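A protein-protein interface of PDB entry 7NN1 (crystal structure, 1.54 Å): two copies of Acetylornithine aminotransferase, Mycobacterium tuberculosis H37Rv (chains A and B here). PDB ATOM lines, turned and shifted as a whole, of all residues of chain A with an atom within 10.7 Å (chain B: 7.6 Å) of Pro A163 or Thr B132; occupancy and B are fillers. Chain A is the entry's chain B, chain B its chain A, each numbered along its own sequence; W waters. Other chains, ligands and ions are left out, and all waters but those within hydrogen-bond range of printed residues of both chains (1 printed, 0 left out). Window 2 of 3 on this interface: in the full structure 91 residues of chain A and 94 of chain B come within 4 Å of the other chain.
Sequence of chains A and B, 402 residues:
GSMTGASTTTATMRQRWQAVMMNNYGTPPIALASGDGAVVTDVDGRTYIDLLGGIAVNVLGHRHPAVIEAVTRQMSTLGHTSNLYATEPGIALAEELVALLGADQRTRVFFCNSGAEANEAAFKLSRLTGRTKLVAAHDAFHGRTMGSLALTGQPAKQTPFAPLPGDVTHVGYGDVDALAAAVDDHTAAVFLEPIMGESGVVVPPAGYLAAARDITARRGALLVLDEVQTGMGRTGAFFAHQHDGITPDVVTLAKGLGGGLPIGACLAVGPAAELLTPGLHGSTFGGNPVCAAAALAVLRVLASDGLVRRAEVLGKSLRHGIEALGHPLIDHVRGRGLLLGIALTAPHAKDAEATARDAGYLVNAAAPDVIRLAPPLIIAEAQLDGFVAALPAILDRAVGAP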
ATOM      1  N   PHE A 123     -32.514 -13.710  -6.853  1.00  0.00           N
ATOM      2  CA  PHE A 123     -31.178 -14.064  -7.336  1.00  0.00           C
ATOM      3  C   PHE A 123     -30.519 -12.862  -8.001  1.00  0.00           C
ATOM      4  O   PHE A 123     -29.368 -12.507  -7.699  1.00  0.00           O
ATOM      5  CB  PHE A 123     -31.297 -15.236  -8.321  1.00  0.00           C
ATOM      6  CG  PHE A 123     -29.986 -15.940  -8.642  1.00  0.00           C
ATOM      7  CD1 PHE A 123     -28.970 -15.288  -9.327  1.00  0.00           C
ATOM      8  CD2 PHE A 123     -29.801 -17.271  -8.312  1.00  0.00           C
ATOM      9  CE1 PHE A 123     -27.781 -15.937  -9.624  1.00  0.00           C
ATOM     10  CE2 PHE A 123     -28.608 -17.928  -8.615  1.00  0.00           C
ATOM     11  CZ  PHE A 123     -27.602 -17.252  -9.271  1.00  0.00           C
ATOM     12  N   ARG A 127     -27.122 -10.342  -7.114  1.00  0.00           N
ATOM     13  CA  ARG A 127     -25.980  -9.996  -7.990  1.00  0.00           C
ATOM     14  C   ARG A 127     -25.635  -8.512  -7.839  1.00  0.00           C
ATOM     15  O   ARG A 127     -24.491  -8.181  -7.928  1.00  0.00           O
ATOM     16  CB  ARG A 127     -26.270 -10.319  -9.455  1.00  0.00           C
ATOM     17  CG  ARG A 127     -26.256 -11.798  -9.782  1.00  0.00           C
ATOM     18  CD  ARG A 127     -24.847 -12.326  -9.939  1.00  0.00           C
ATOM     19  NE  ARG A 127     -24.734 -13.596 -10.607  1.00  0.00           N
ATOM     20  CZ  ARG A 127     -24.479 -14.756 -10.034  1.00  0.00           C
ATOM     21  NH1 ARG A 127     -24.368 -14.848  -8.731  1.00  0.00           N
ATOM     22  NH2 ARG A 127     -24.353 -15.830 -10.770  1.00  0.00           N
ATOM     23  N   THR A 145     -36.399 -23.036 -12.752  1.00  0.00           N
ATOM     24  CA  THR A 145     -35.703 -22.220 -13.778  1.00  0.00           C
ATOM     25  C   THR A 145     -34.185 -22.264 -13.501  1.00  0.00           C
ATOM     26  O   THR A 145     -33.806 -22.582 -12.428  1.00  0.00           O
ATOM     27  CB  THR A 145     -36.296 -20.809 -13.883  1.00  0.00           C
ATOM     28  OG1 THR A 145     -36.272 -20.199 -12.603  1.00  0.00           O
ATOM     29  CG2 THR A 145     -37.707 -20.829 -14.424  1.00  0.00           C
ATOM     30  N   MET A 146     -33.348 -21.890 -14.462  1.00  0.00           N
ATOM     31  CA  MET A 146     -31.878 -22.069 -14.296  1.00  0.00           C
ATOM     32  C   MET A 146     -31.310 -21.412 -13.031  1.00  0.00           C
ATOM     33  O   MET A 146     -30.506 -22.030 -12.373  1.00  0.00           O
ATOM     34  CB  MET A 146     -31.093 -21.677 -15.550  1.00  0.00           C
ATOM     35  CG  MET A 146     -31.392 -22.578 -16.730  1.00  0.00           C
ATOM     36  SD  MET A 146     -30.782 -24.267 -16.484  1.00  0.00           S
ATOM     37  CE  MET A 146     -29.019 -23.955 -16.500  1.00  0.00           C
ATOM     38  N   GLY A 147     -31.758 -20.212 -12.698  1.00  0.00           N
ATOM     39  CA  GLY A 147     -31.267 -19.571 -11.486  1.00  0.00           C
ATOM     40  C   GLY A 147     -31.830 -20.196 -10.220  1.00  0.00           C
ATOM     41  O   GLY A 147     -31.092 -20.549  -9.289  1.00  0.00           O
ATOM     42  N   LEU A 149     -33.056 -23.077  -9.898  1.00  0.00           N
ATOM     43  CA  LEU A 149     -32.614 -24.469  -9.808  1.00  0.00           C
ATOM     44  C   LEU A 149     -31.215 -24.582  -9.205  1.00  0.00           C
ATOM     45  O   LEU A 149     -30.900 -25.581  -8.546  1.00  0.00           O
ATOM     46  CB  LEU A 149     -32.646 -25.122 -11.192  1.00  0.00           C
ATOM     47  CG  LEU A 149     -32.344 -26.616 -11.304  1.00  0.00           C
ATOM     48  CD1 LEU A 149     -33.314 -27.453 -10.477  1.00  0.00           C
ATOM     49  CD2 LEU A 149     -32.405 -27.034 -12.773  1.00  0.00           C
ATOM     50  N   ALA A 150     -30.367 -23.572  -9.424  1.00  0.00           N
ATOM     51  CA  ALA A 150     -29.057 -23.555  -8.782  1.00  0.00           C
ATOM     52  C   ALA A 150     -29.188 -23.452  -7.268  1.00  0.00           C
ATOM     53  O   ALA A 150     -28.361 -23.999  -6.528  1.00  0.00           O
ATOM     54  CB  ALA A 150     -28.236 -22.391  -9.325  1.00  0.00           C
ATOM     55  N   LEU A 151     -30.211 -22.737  -6.794  1.00  0.00           N
ATOM     56  CA  LEU A 151     -30.458 -22.578  -5.360  1.00  0.00           C
ATOM     57  C   LEU A 151     -31.109 -23.816  -4.769  1.00  0.00           C
ATOM     58  O   LEU A 151     -30.828 -24.191  -3.626  1.00  0.00           O
ATOM     59  CB  LEU A 151     -31.362 -21.367  -5.111  1.00  0.00           C
ATOM     60  CG  LEU A 151     -30.819 -20.004  -5.541  1.00  0.00           C
ATOM     61  CD1 LEU A 151     -31.958 -18.990  -5.520  1.00  0.00           C
ATOM     62  CD2 LEU A 151     -29.687 -19.584  -4.629  1.00  0.00           C
ATOM     63  N   LYS A 157     -32.478 -33.285  -9.510  1.00  0.00           N
ATOM     64  CA  LYS A 157     -33.183 -32.320 -10.385  1.00  0.00           C
ATOM     65  C   LYS A 157     -32.180 -31.364 -11.055  1.00  0.00           C
ATOM     66  O   LYS A 157     -32.563 -30.726 -11.987  1.00  0.00           O
ATOM     67  CB  LYS A 157     -34.158 -31.468  -9.565  1.00  0.00           C
ATOM     68  CG  LYS A 157     -35.351 -32.130  -8.876  1.00  0.00           C
ATOM     69  CD  LYS A 157     -36.021 -31.134  -7.933  1.00  0.00           C
ATOM     70  CE  LYS A 157     -37.527 -31.138  -7.835  1.00  0.00           C
ATOM     71  NZ  LYS A 157     -37.996 -31.857  -6.629  1.00  0.00           N
ATOM     72  N   GLN A 158     -30.948 -31.285 -10.563  1.00  0.00           N
ATOM     73  CA  GLN A 158     -29.963 -30.317 -11.032  1.00  0.00           C
ATOM     74  C   GLN A 158     -28.963 -30.903 -12.020  1.00  0.00           C
ATOM     75  O   GLN A 158     -28.674 -30.274 -13.043  1.00  0.00           O
ATOM     76  CB  GLN A 158     -29.183 -29.739  -9.854  1.00  0.00           C
ATOM     77  CG  GLN A 158     -30.013 -29.092  -8.772  1.00  0.00           C
ATOM     78  CD  GLN A 158     -29.150 -28.663  -7.610  1.00  0.00           C
ATOM     79  OE1 GLN A 158     -28.626 -29.503  -6.860  1.00  0.00           O
ATOM     80  NE2 GLN A 158     -28.985 -27.365  -7.451  1.00  0.00           N
ATOM     81  N   THR A 159     -28.416 -32.084 -11.708  1.00  0.00           N
ATOM     82  CA  THR A 159     -27.315 -32.675 -12.470  1.00  0.00           C
ATOM     83  C   THR A 159     -27.534 -32.716 -13.979  1.00  0.00           C
ATOM     84  O   THR A 159     -26.605 -32.337 -14.716  1.00  0.00           O
ATOM     85  CB  THR A 159     -27.029 -34.077 -11.915  1.00  0.00           C
ATOM     86  OG1 THR A 159     -26.438 -33.945 -10.619  1.00  0.00           O
ATOM     87  CG2 THR A 159     -26.074 -34.840 -12.838  1.00  0.00           C
ATOM     88  N   PRO A 160     -28.686 -33.153 -14.510  1.00  0.00           N
ATOM     89  CA  PRO A 160     -28.829 -33.207 -15.972  1.00  0.00           C
ATOM     90  C   PRO A 160     -28.743 -31.849 -16.640  1.00  0.00           C
ATOM     91  O   PRO A 160     -28.612 -31.797 -17.869  1.00  0.00           O
ATOM     92  CB  PRO A 160     -30.216 -33.833 -16.182  1.00  0.00           C
ATOM     93  CG  PRO A 160     -30.562 -34.481 -14.863  1.00  0.00           C
ATOM     94  CD  PRO A 160     -29.908 -33.623 -13.831  1.00  0.00           C
ATOM     95  N   PHE A 161     -28.806 -30.779 -15.852  1.00  0.00           N
ATOM     96  CA  PHE A 161     -28.868 -29.419 -16.431  1.00  0.00           C
ATOM     97  C   PHE A 161     -27.586 -28.632 -16.180  1.00  0.00           C
ATOM     98  O   PHE A 161     -27.533 -27.507 -16.564  1.00  0.00           O
ATOM     99  CB  PHE A 161     -30.113 -28.693 -15.906  1.00  0.00           C
ATOM    100  CG  PHE A 161     -31.358 -29.485 -16.172  1.00  0.00           C
ATOM    101  CD1 PHE A 161     -31.840 -29.606 -17.459  1.00  0.00           C
ATOM    102  CD2 PHE A 161     -31.990 -30.186 -15.172  1.00  0.00           C
ATOM    103  CE1 PHE A 161     -32.945 -30.382 -17.728  1.00  0.00           C
ATOM    104  CE2 PHE A 161     -33.094 -30.961 -15.448  1.00  0.00           C
ATOM    105  CZ  PHE A 161     -33.569 -31.054 -16.719  1.00  0.00           C
ATOM    106  N   ALA A 162     -26.591 -29.249 -15.554  1.00  0.00           N
ATOM    107  CA  ALA A 162     -25.327 -28.535 -15.287  1.00  0.00           C
ATOM    108  C   ALA A 162     -24.628 -28.165 -16.595  1.00  0.00           C
ATOM    109  O   ALA A 162     -24.715 -28.904 -17.556  1.00  0.00           O
ATOM    110  CB  ALA A 162     -24.433 -29.358 -14.413  1.00  0.00           C
ATOM    111  N   PRO A 163     -23.859 -27.071 -16.630  1.00  0.00           N
ATOM    112  CA  PRO A 163     -23.664 -26.222 -15.470  1.00  0.00           C
ATOM    113  C   PRO A 163     -24.761 -25.187 -15.167  1.00  0.00           C
ATOM    114  O   PRO A 163     -25.254 -24.594 -16.033  1.00  0.00           O
ATOM    115  CB  PRO A 163     -22.377 -25.482 -15.832  1.00  0.00           C
ATOM    116  CG  PRO A 163     -22.439 -25.374 -17.318  1.00  0.00           C
ATOM    117  CD  PRO A 163     -23.076 -26.661 -17.774  1.00  0.00           C
ATOM    118  N   LEU A 164     -25.049 -25.006 -13.889  1.00  0.00           N
ATOM    119  CA  LEU A 164     -26.044 -24.006 -13.442  1.00  0.00           C
ATOM    120  C   LEU A 164     -25.321 -22.726 -13.019  1.00  0.00           C
ATOM    121  O   LEU A 164     -24.149 -22.788 -12.745  1.00  0.00           O
ATOM    122  CB  LEU A 164     -26.818 -24.575 -12.253  1.00  0.00           C
ATOM    123  CG  LEU A 164     -27.590 -25.863 -12.512  1.00  0.00           C
ATOM    124  CD1 LEU A 164     -28.315 -26.323 -11.263  1.00  0.00           C
ATOM    125  CD2 LEU A 164     -28.570 -25.694 -13.642  1.00  0.00           C
ATOM    126  N   PRO A 165     -26.015 -21.580 -12.933  1.00  0.00           N
ATOM    127  CA  PRO A 165     -25.392 -20.333 -12.503  1.00  0.00           C
ATOM    128  C   PRO A 165     -24.778 -20.444 -11.098  1.00  0.00           C
ATOM    129  O   PRO A 165     -25.326 -21.072 -10.267  1.00  0.00           O
ATOM    130  CB  PRO A 165     -26.496 -19.289 -12.557  1.00  0.00           C
ATOM    131  CG  PRO A 165     -27.758 -20.058 -12.751  1.00  0.00           C
ATOM    132  CD  PRO A 165     -27.403 -21.416 -13.302  1.00  0.00           C
ATOM    133  N   GLY A 166     -23.644 -19.786 -10.904  1.00  0.00           N
ATOM    134  CA  GLY A 166     -22.887 -19.917  -9.647  1.00  0.00           C
ATOM    135  C   GLY A 166     -23.059 -18.727  -8.747  1.00  0.00           C
ATOM    136  O   GLY A 166     -23.803 -17.863  -9.104  1.00  0.00           O
ATOM    137  N   ASP A 167     -22.343 -18.696  -7.631  1.00  0.00           N
ATOM    138  CA  ASP A 167     -21.573 -19.834  -7.068  1.00  0.00           C
ATOM    139  C   ASP A 167     -22.285 -20.253  -5.780  1.00  0.00           C
ATOM    140  O   ASP A 167     -22.175 -19.567  -4.793  1.00  0.00           O
ATOM    141  CB  ASP A 167     -20.117 -19.442  -6.819  1.00  0.00           C
ATOM    142  CG  ASP A 167     -19.345 -19.080  -8.076  1.00  0.00           C
ATOM    143  OD1 ASP A 167     -19.478 -19.784  -9.050  1.00  0.00           O
ATOM    144  OD2 ASP A 167     -18.650 -18.089  -8.056  1.00  0.00           O
ATOM    145  N   VAL A 168     -22.978 -21.379  -5.831  1.00  0.00           N
ATOM    146  CA  VAL A 168     -23.859 -21.788  -4.709  1.00  0.00           C
ATOM    147  C   VAL A 168     -23.234 -22.867  -3.839  1.00  0.00           C
ATOM    148  O   VAL A 168     -22.763 -23.843  -4.371  1.00  0.00           O
ATOM    149  CB  VAL A 168     -25.204 -22.287  -5.261  1.00  0.00           C
ATOM    150  CG1 VAL A 168     -26.198 -22.542  -4.152  1.00  0.00           C
ATOM    151  CG2 VAL A 168     -25.778 -21.331  -6.290  1.00  0.00           C
ATOM    152  N   PHE B 123     -34.199 -24.015 -22.810  1.00  0.00           N
ATOM    153  CA  PHE B 123     -32.803 -24.056 -22.377  1.00  0.00           C
ATOM    154  C   PHE B 123     -32.482 -25.394 -21.702  1.00  0.00           C
ATOM    155  O   PHE B 123     -31.471 -26.047 -22.010  1.00  0.00           O
ATOM    156  CB  PHE B 123     -32.563 -22.880 -21.420  1.00  0.00           C
ATOM    157  CG  PHE B 123     -31.110 -22.596 -21.094  1.00  0.00           C
ATOM    158  CD1 PHE B 123     -30.320 -23.521 -20.417  1.00  0.00           C
ATOM    159  CD2 PHE B 123     -30.560 -21.368 -21.408  1.00  0.00           C
ATOM    160  CE1 PHE B 123     -28.996 -23.232 -20.101  1.00  0.00           C
ATOM    161  CE2 PHE B 123     -29.235 -21.073 -21.095  1.00  0.00           C
ATOM    162  CZ  PHE B 123     -28.454 -22.020 -20.444  1.00  0.00           C
ATOM    163  N   SER B 126     -32.272 -28.189 -24.039  1.00  0.00           N
ATOM    164  CA  SER B 126     -31.016 -28.203 -24.784  1.00  0.00           C
ATOM    165  C   SER B 126     -29.902 -28.867 -23.987  1.00  0.00           C
ATOM    166  O   SER B 126     -29.001 -29.469 -24.579  1.00  0.00           O
ATOM    167  CB  SER B 126     -30.604 -26.786 -25.186  1.00  0.00           C
ATOM    168  OG  SER B 126     -29.931 -26.114 -24.136  1.00  0.00           O
ATOM    169  N   ARG B 127     -29.945 -28.764 -22.657  1.00  0.00           N
ATOM    170  CA  ARG B 127     -28.976 -29.480 -21.830  1.00  0.00           C
ATOM    171  C   ARG B 127     -29.072 -30.986 -22.032  1.00  0.00           C
ATOM    172  O   ARG B 127     -28.056 -31.689 -21.976  1.00  0.00           O
ATOM    173  CB  ARG B 127     -29.186 -29.143 -20.351  1.00  0.00           C
ATOM    174  CG  ARG B 127     -28.701 -27.750 -19.945  1.00  0.00           C
ATOM    175  CD  ARG B 127     -27.175 -27.664 -19.918  1.00  0.00           C
ATOM    176  NE  ARG B 127     -26.671 -26.523 -19.151  1.00  0.00           N
ATOM    177  CZ  ARG B 127     -26.114 -25.439 -19.678  1.00  0.00           C
ATOM    178  NH1 ARG B 127     -26.004 -25.313 -20.997  1.00  0.00           N
ATOM    179  NH2 ARG B 127     -25.661 -24.473 -18.891  1.00  0.00           N
ATOM    180  N   THR B 129     -29.448 -32.674 -24.602  1.00  0.00           N
ATOM    181  CA  THR B 129     -28.749 -33.144 -25.792  1.00  0.00           C
ATOM    182  C   THR B 129     -27.339 -33.630 -25.502  1.00  0.00           C
ATOM    183  O   THR B 129     -26.692 -34.171 -26.406  1.00  0.00           O
ATOM    184  CB  THR B 129     -28.642 -32.034 -26.838  1.00  0.00           C
ATOM    185  OG1 THR B 129     -27.751 -31.018 -26.352  1.00  0.00           O
ATOM    186  CG2 THR B 129     -30.001 -31.433 -27.124  1.00  0.00           C
ATOM    187  N   GLY B 130     -26.832 -33.411 -24.296  1.00  0.00           N
ATOM    188  CA  GLY B 130     -25.450 -33.697 -23.989  1.00  0.00           C
ATOM    189  C   GLY B 130     -24.482 -32.587 -24.323  1.00  0.00           C
ATOM    190  O   GLY B 130     -23.278 -32.746 -24.082  1.00  0.00           O
ATOM    191  N   ARG B 131     -24.958 -31.482 -24.888  1.00  0.00           N
ATOM    192  CA  ARG B 131     -24.117 -30.350 -25.233  1.00  0.00           C
ATOM    193  C   ARG B 131     -24.505 -29.140 -24.393  1.00  0.00           C
ATOM    194  O   ARG B 131     -25.651 -29.014 -23.948  1.00  0.00           O
ATOM    195  CB  ARG B 131     -24.241 -30.004 -26.728  1.00  0.00           C
ATOM    196  CG  ARG B 131     -23.998 -31.180 -27.669  1.00  0.00           C
ATOM    197  CD  ARG B 131     -24.469 -30.857 -29.099  1.00  0.00           C
ATOM    198  NE  ARG B 131     -24.169 -31.943 -30.031  1.00  0.00           N
ATOM    199  CZ  ARG B 131     -24.103 -31.802 -31.351  1.00  0.00           C
ATOM    200  NH1 ARG B 131     -24.320 -30.611 -31.902  1.00  0.00           N
ATOM    201  NH2 ARG B 131     -23.813 -32.847 -32.118  1.00  0.00           N
ATOM    202  N   THR B 132     -23.541 -28.243 -24.188  1.00  0.00           N
ATOM    203  CA  THR B 132     -23.741 -27.061 -23.359  1.00  0.00           C
ATOM    204  C   THR B 132     -23.517 -25.749 -24.101  1.00  0.00           C
ATOM    205  O   THR B 132     -23.700 -24.679 -23.509  1.00  0.00           O
ATOM    206  CB  THR B 132     -22.811 -27.101 -22.140  1.00  0.00           C
ATOM    207  OG1 THR B 132     -21.458 -27.097 -22.596  1.00  0.00           O
ATOM    208  CG2 THR B 132     -23.065 -28.361 -21.298  1.00  0.00           C
ATOM    209  N   LYS B 133     -23.122 -25.795 -25.369  1.00  0.00           N
ATOM    210  CA  LYS B 133     -22.881 -24.590 -26.153  1.00  0.00           C
ATOM    211  C   LYS B 133     -24.178 -24.139 -26.812  1.00  0.00           C
ATOM    212  O   LYS B 133     -24.915 -24.965 -27.362  1.00  0.00           O
ATOM    213  CB  LYS B 133     -21.815 -24.862 -27.213  1.00  0.00           C
ATOM    214  CG  LYS B 133     -21.363 -23.647 -27.965  1.00  0.00           C
ATOM    215  CD  LYS B 133     -20.632 -24.014 -29.253  1.00  0.00           C
ATOM    216  CE  LYS B 133     -21.015 -23.036 -30.353  1.00  0.00           C
ATOM    217  NZ  LYS B 133     -20.143 -21.833 -30.308  1.00  0.00           N
ATOM    218  N   LEU B 134     -24.461 -22.836 -26.744  1.00  0.00           N
ATOM    219  CA  LEU B 134     -25.684 -22.266 -27.297  1.00  0.00           C
ATOM    220  C   LEU B 134     -25.353 -21.046 -28.138  1.00  0.00           C
ATOM    221  O   LEU B 134     -24.378 -20.341 -27.876  1.00  0.00           O
ATOM    222  CB  LEU B 134     -26.662 -21.842 -26.203  1.00  0.00           C
ATOM    223  CG  LEU B 134     -27.116 -22.986 -25.290  1.00  0.00           C
ATOM    224  CD1 LEU B 134     -27.350 -22.474 -23.882  1.00  0.00           C
ATOM    225  CD2 LEU B 134     -28.359 -23.624 -25.858  1.00  0.00           C
ATOM    226  N   VAL B 135     -26.196 -20.776 -29.138  1.00  0.00           N
ATOM    227  CA  VAL B 135     -26.004 -19.641 -30.034  1.00  0.00           C
ATOM    228  C   VAL B 135     -27.300 -18.845 -30.089  1.00  0.00           C
ATOM    229  O   VAL B 135     -28.383 -19.424 -30.219  1.00  0.00           O
ATOM    230  CB  VAL B 135     -25.588 -20.079 -31.454  1.00  0.00           C
ATOM    231  CG1 VAL B 135     -25.421 -18.850 -32.387  1.00  0.00           C
ATOM    232  CG2 VAL B 135     -24.300 -20.890 -31.404  1.00  0.00           C
ATOM    233  N   LEU B 164     -23.657 -15.444 -15.940  1.00  0.00           N
ATOM    234  CA  LEU B 164     -24.936 -16.055 -16.355  1.00  0.00           C
ATOM    235  C   LEU B 164     -24.679 -17.499 -16.770  1.00  0.00           C
ATOM    236  O   LEU B 164     -23.562 -17.836 -17.062  1.00  0.00           O
ATOM    237  CB  LEU B 164     -25.488 -15.272 -17.541  1.00  0.00           C
ATOM    238  CG  LEU B 164     -25.851 -13.819 -17.279  1.00  0.00           C
ATOM    239  CD1 LEU B 164     -26.443 -13.192 -18.513  1.00  0.00           C
ATOM    240  CD2 LEU B 164     -26.828 -13.700 -16.140  1.00  0.00           C
ATOM    241  N   PRO B 165     -25.708 -18.350 -16.845  1.00  0.00           N
ATOM    242  CA  PRO B 165     -25.523 -19.710 -17.314  1.00  0.00           C
ATOM    243  C   PRO B 165     -24.874 -19.729 -18.714  1.00  0.00           C
ATOM    244  O   PRO B 165     -25.245 -18.959 -19.548  1.00  0.00           O
ATOM    245  CB  PRO B 165     -26.953 -20.242 -17.431  1.00  0.00           C
ATOM    246  CG  PRO B 165     -27.774 -19.370 -16.543  1.00  0.00           C
ATOM    247  CD  PRO B 165     -27.060 -18.048 -16.428  1.00  0.00           C
ATOM    248  N   GLY B 166     -23.957 -20.668 -18.936  1.00  0.00           N
ATOM    249  CA  GLY B 166     -23.241 -20.757 -20.220  1.00  0.00           C
ATOM    250  C   GLY B 166     -23.675 -21.919 -21.083  1.00  0.00           C
ATOM    251  O   GLY B 166     -24.567 -22.618 -20.716  1.00  0.00           O
ATOM    252  N   ASP B 167     -23.002 -22.132 -22.207  1.00  0.00           N
ATOM    253  CA  ASP B 167     -21.968 -21.241 -22.778  1.00  0.00           C
ATOM    254  C   ASP B 167     -22.576 -20.652 -24.052  1.00  0.00           C
ATOM    255  O   ASP B 167     -22.761 -21.360 -24.993  1.00  0.00           O
ATOM    256  CB  ASP B 167     -20.699 -22.033 -23.070  1.00  0.00           C
ATOM    257  CG  ASP B 167     -20.078 -22.646 -21.831  1.00  0.00           C
ATOM    258  OD1 ASP B 167     -20.153 -22.019 -20.783  1.00  0.00           O
ATOM    259  OD2 ASP B 167     -19.504 -23.728 -21.944  1.00  0.00           O
ATOM    260  N   VAL B 168     -22.884 -19.372 -24.021  1.00  0.00           N
ATOM    261  CA  VAL B 168     -23.658 -18.773 -25.131  1.00  0.00           C
ATOM    262  C   VAL B 168     -22.784 -17.859 -25.965  1.00  0.00           C
ATOM    263  O   VAL B 168     -22.112 -17.040 -25.403  1.00  0.00           O
ATOM    264  CB  VAL B 168     -24.873 -17.979 -24.612  1.00  0.00           C
ATOM    265  CG1 VAL B 168     -25.785 -17.581 -25.749  1.00  0.00           C
ATOM    266  CG2 VAL B 168     -25.625 -18.708 -23.516  1.00  0.00           C
ATOM    267  N   HIS B 186     -20.540 -29.154 -31.248  1.00  0.00           N
ATOM    268  CA  HIS B 186     -20.720 -29.053 -29.808  1.00  0.00           C
ATOM    269  C   HIS B 186     -21.884 -28.148 -29.429  1.00  0.00           C
ATOM    270  O   HIS B 186     -22.121 -27.914 -28.238  1.00  0.00           O
ATOM    271  CB  HIS B 186     -19.422 -28.560 -29.163  1.00  0.00           C
ATOM    272  CG  HIS B 186     -18.271 -29.491 -29.376  1.00  0.00           C
ATOM    273  ND1 HIS B 186     -17.053 -29.072 -29.865  1.00  0.00           N
ATOM    274  CD2 HIS B 186     -18.162 -30.828 -29.186  1.00  0.00           C
ATOM    275  CE1 HIS B 186     -16.240 -30.109 -29.961  1.00  0.00           C
ATOM    276  NE2 HIS B 186     -16.888 -31.186 -29.555  1.00  0.00           N
ATOM    277  N   THR B 187     -22.631 -27.656 -30.407  1.00  0.00           N
ATOM    278  CA  THR B 187     -23.707 -26.704 -30.165  1.00  0.00           C
ATOM    279  C   THR B 187     -24.985 -27.451 -29.808  1.00  0.00           C
ATOM    280  O   THR B 187     -25.482 -28.264 -30.599  1.00  0.00           O
ATOM    281  CB  THR B 187     -23.911 -25.828 -31.403  1.00  0.00           C
ATOM    282  OG1 THR B 187     -22.688 -25.136 -31.694  1.00  0.00           O
ATOM    283  CG2 THR B 187     -25.029 -24.810 -31.165  1.00  0.00           C
ATOM    284  N   ALA B 188     -25.525 -27.167 -28.616  1.00  0.00           N
ATOM    285  CA  ALA B 188     -26.775 -27.790 -28.194  1.00  0.00           C
ATOM    286  C   ALA B 188     -27.960 -27.232 -28.970  1.00  0.00           C
ATOM    287  O   ALA B 188     -28.842 -27.982 -29.406  1.00  0.00           O
ATOM    288  CB  ALA B 188     -26.994 -27.583 -26.692  1.00  0.00           C
ATOM    289  N   ALA B 189     -28.016 -25.914 -29.126  1.00  0.00           N
ATOM    290  CA  ALA B 189     -29.203 -25.302 -29.701  1.00  0.00           C
ATOM    291  C   ALA B 189     -28.876 -23.909 -30.192  1.00  0.00           C
ATOM    292  O   ALA B 189     -27.957 -23.257 -29.686  1.00  0.00           O
ATOM    293  CB  ALA B 189     -30.351 -25.240 -28.682  1.00  0.00           C
HETATM  294  O   HOH W   1     -24.037 -22.408 -16.552  1.00  0.00           O
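Pro B165 touches its own counterpart, Pro A165. Positions printed for both chains: 123, 127, 164, 165, 166, 167 and 168.
N of Asp B167 is in hydrogen-bond range of O of Thr B132, at 2.9 Å. The guanidinium group (NH1) of Arg B127 is in hydrogen-bond range of the backbone carbonyl oxygen (O) of Thr B132 (3.5 Å). O of Phe B123 is in hydrogen-bond range of OG of Ser B126, at 2.6 Å. NH2 of Arg B127 lies within hydrogen-bond range of O of Gly B166 (2.8 Å).
Met A146 touches Phe B123 (CE to CE1, 3.7 Å). O of Pro A160 touches CB of Arg B127 (3.7 Å). Pro A163 touches Thr B132 (CD to CG2, 3.9 Å). Pro B165 touches Pro A165 (CG to CD, 3.9 Å).
The guanidinium group (NE) of Arg B127 is in hydrogen-bond range of the backbone carbonyl oxygen (O) of Phe A161 (2.9 Å). NH2 of Arg B127 sits at hydrogen-bond distance from O of Pro A163 (2.9 Å). The guanidinium group of Arg B127 lies within hydrogen-bond range of the backbone carbonyl oxygen of Ala A162 (3.5 Å).
Water W1 bridges the backbone carbonyl oxygen (O) of Pro A163 (2.6 Å) and the backbone NH (N) of Gly B166 (3.0 Å).
Pro A163 touches just these residues of chain B: Arg B127 (2.9 Å) and Thr B132 (3.9 Å). Of chain A, only Pro A163 comes within 4 Å of Thr B132. Of chain A, only Pro A160 (3.7 Å), Phe A161 (2.9 Å), Ala A162 (3.5 Å) and Pro A163 (2.9 Å) come within 4 Å of Arg B127. No residue of chain A comes within 4 Å of Gly B130. No residue of chain A comes within 4 Å of Leu B134. No residue of chain A comes within 4 Å of Asp B167. Printed residues of chain A within 4 Å of Phe B123: Met A146 (3.7 Å). Of the printed residues of chain B, Pro A160 touches Arg B127. Printed residues of chain B within 4 Å of Met A146: Phe B123 (3.7 Å). Of the printed residues of chain A, Pro B165 touches Pro A165 (3.9 Å). The nearest printed residue of chain B that does not touch Pro A165 is Leu B164 (4.9 Å).
Of the 19 printed residues of chain B, 4 touch a printed residue of chain A. Among the printed residues, no Asp or Glu carboxylate lies within 4 Å of a Lys or Arg side-chain nitrogen of the other chain.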
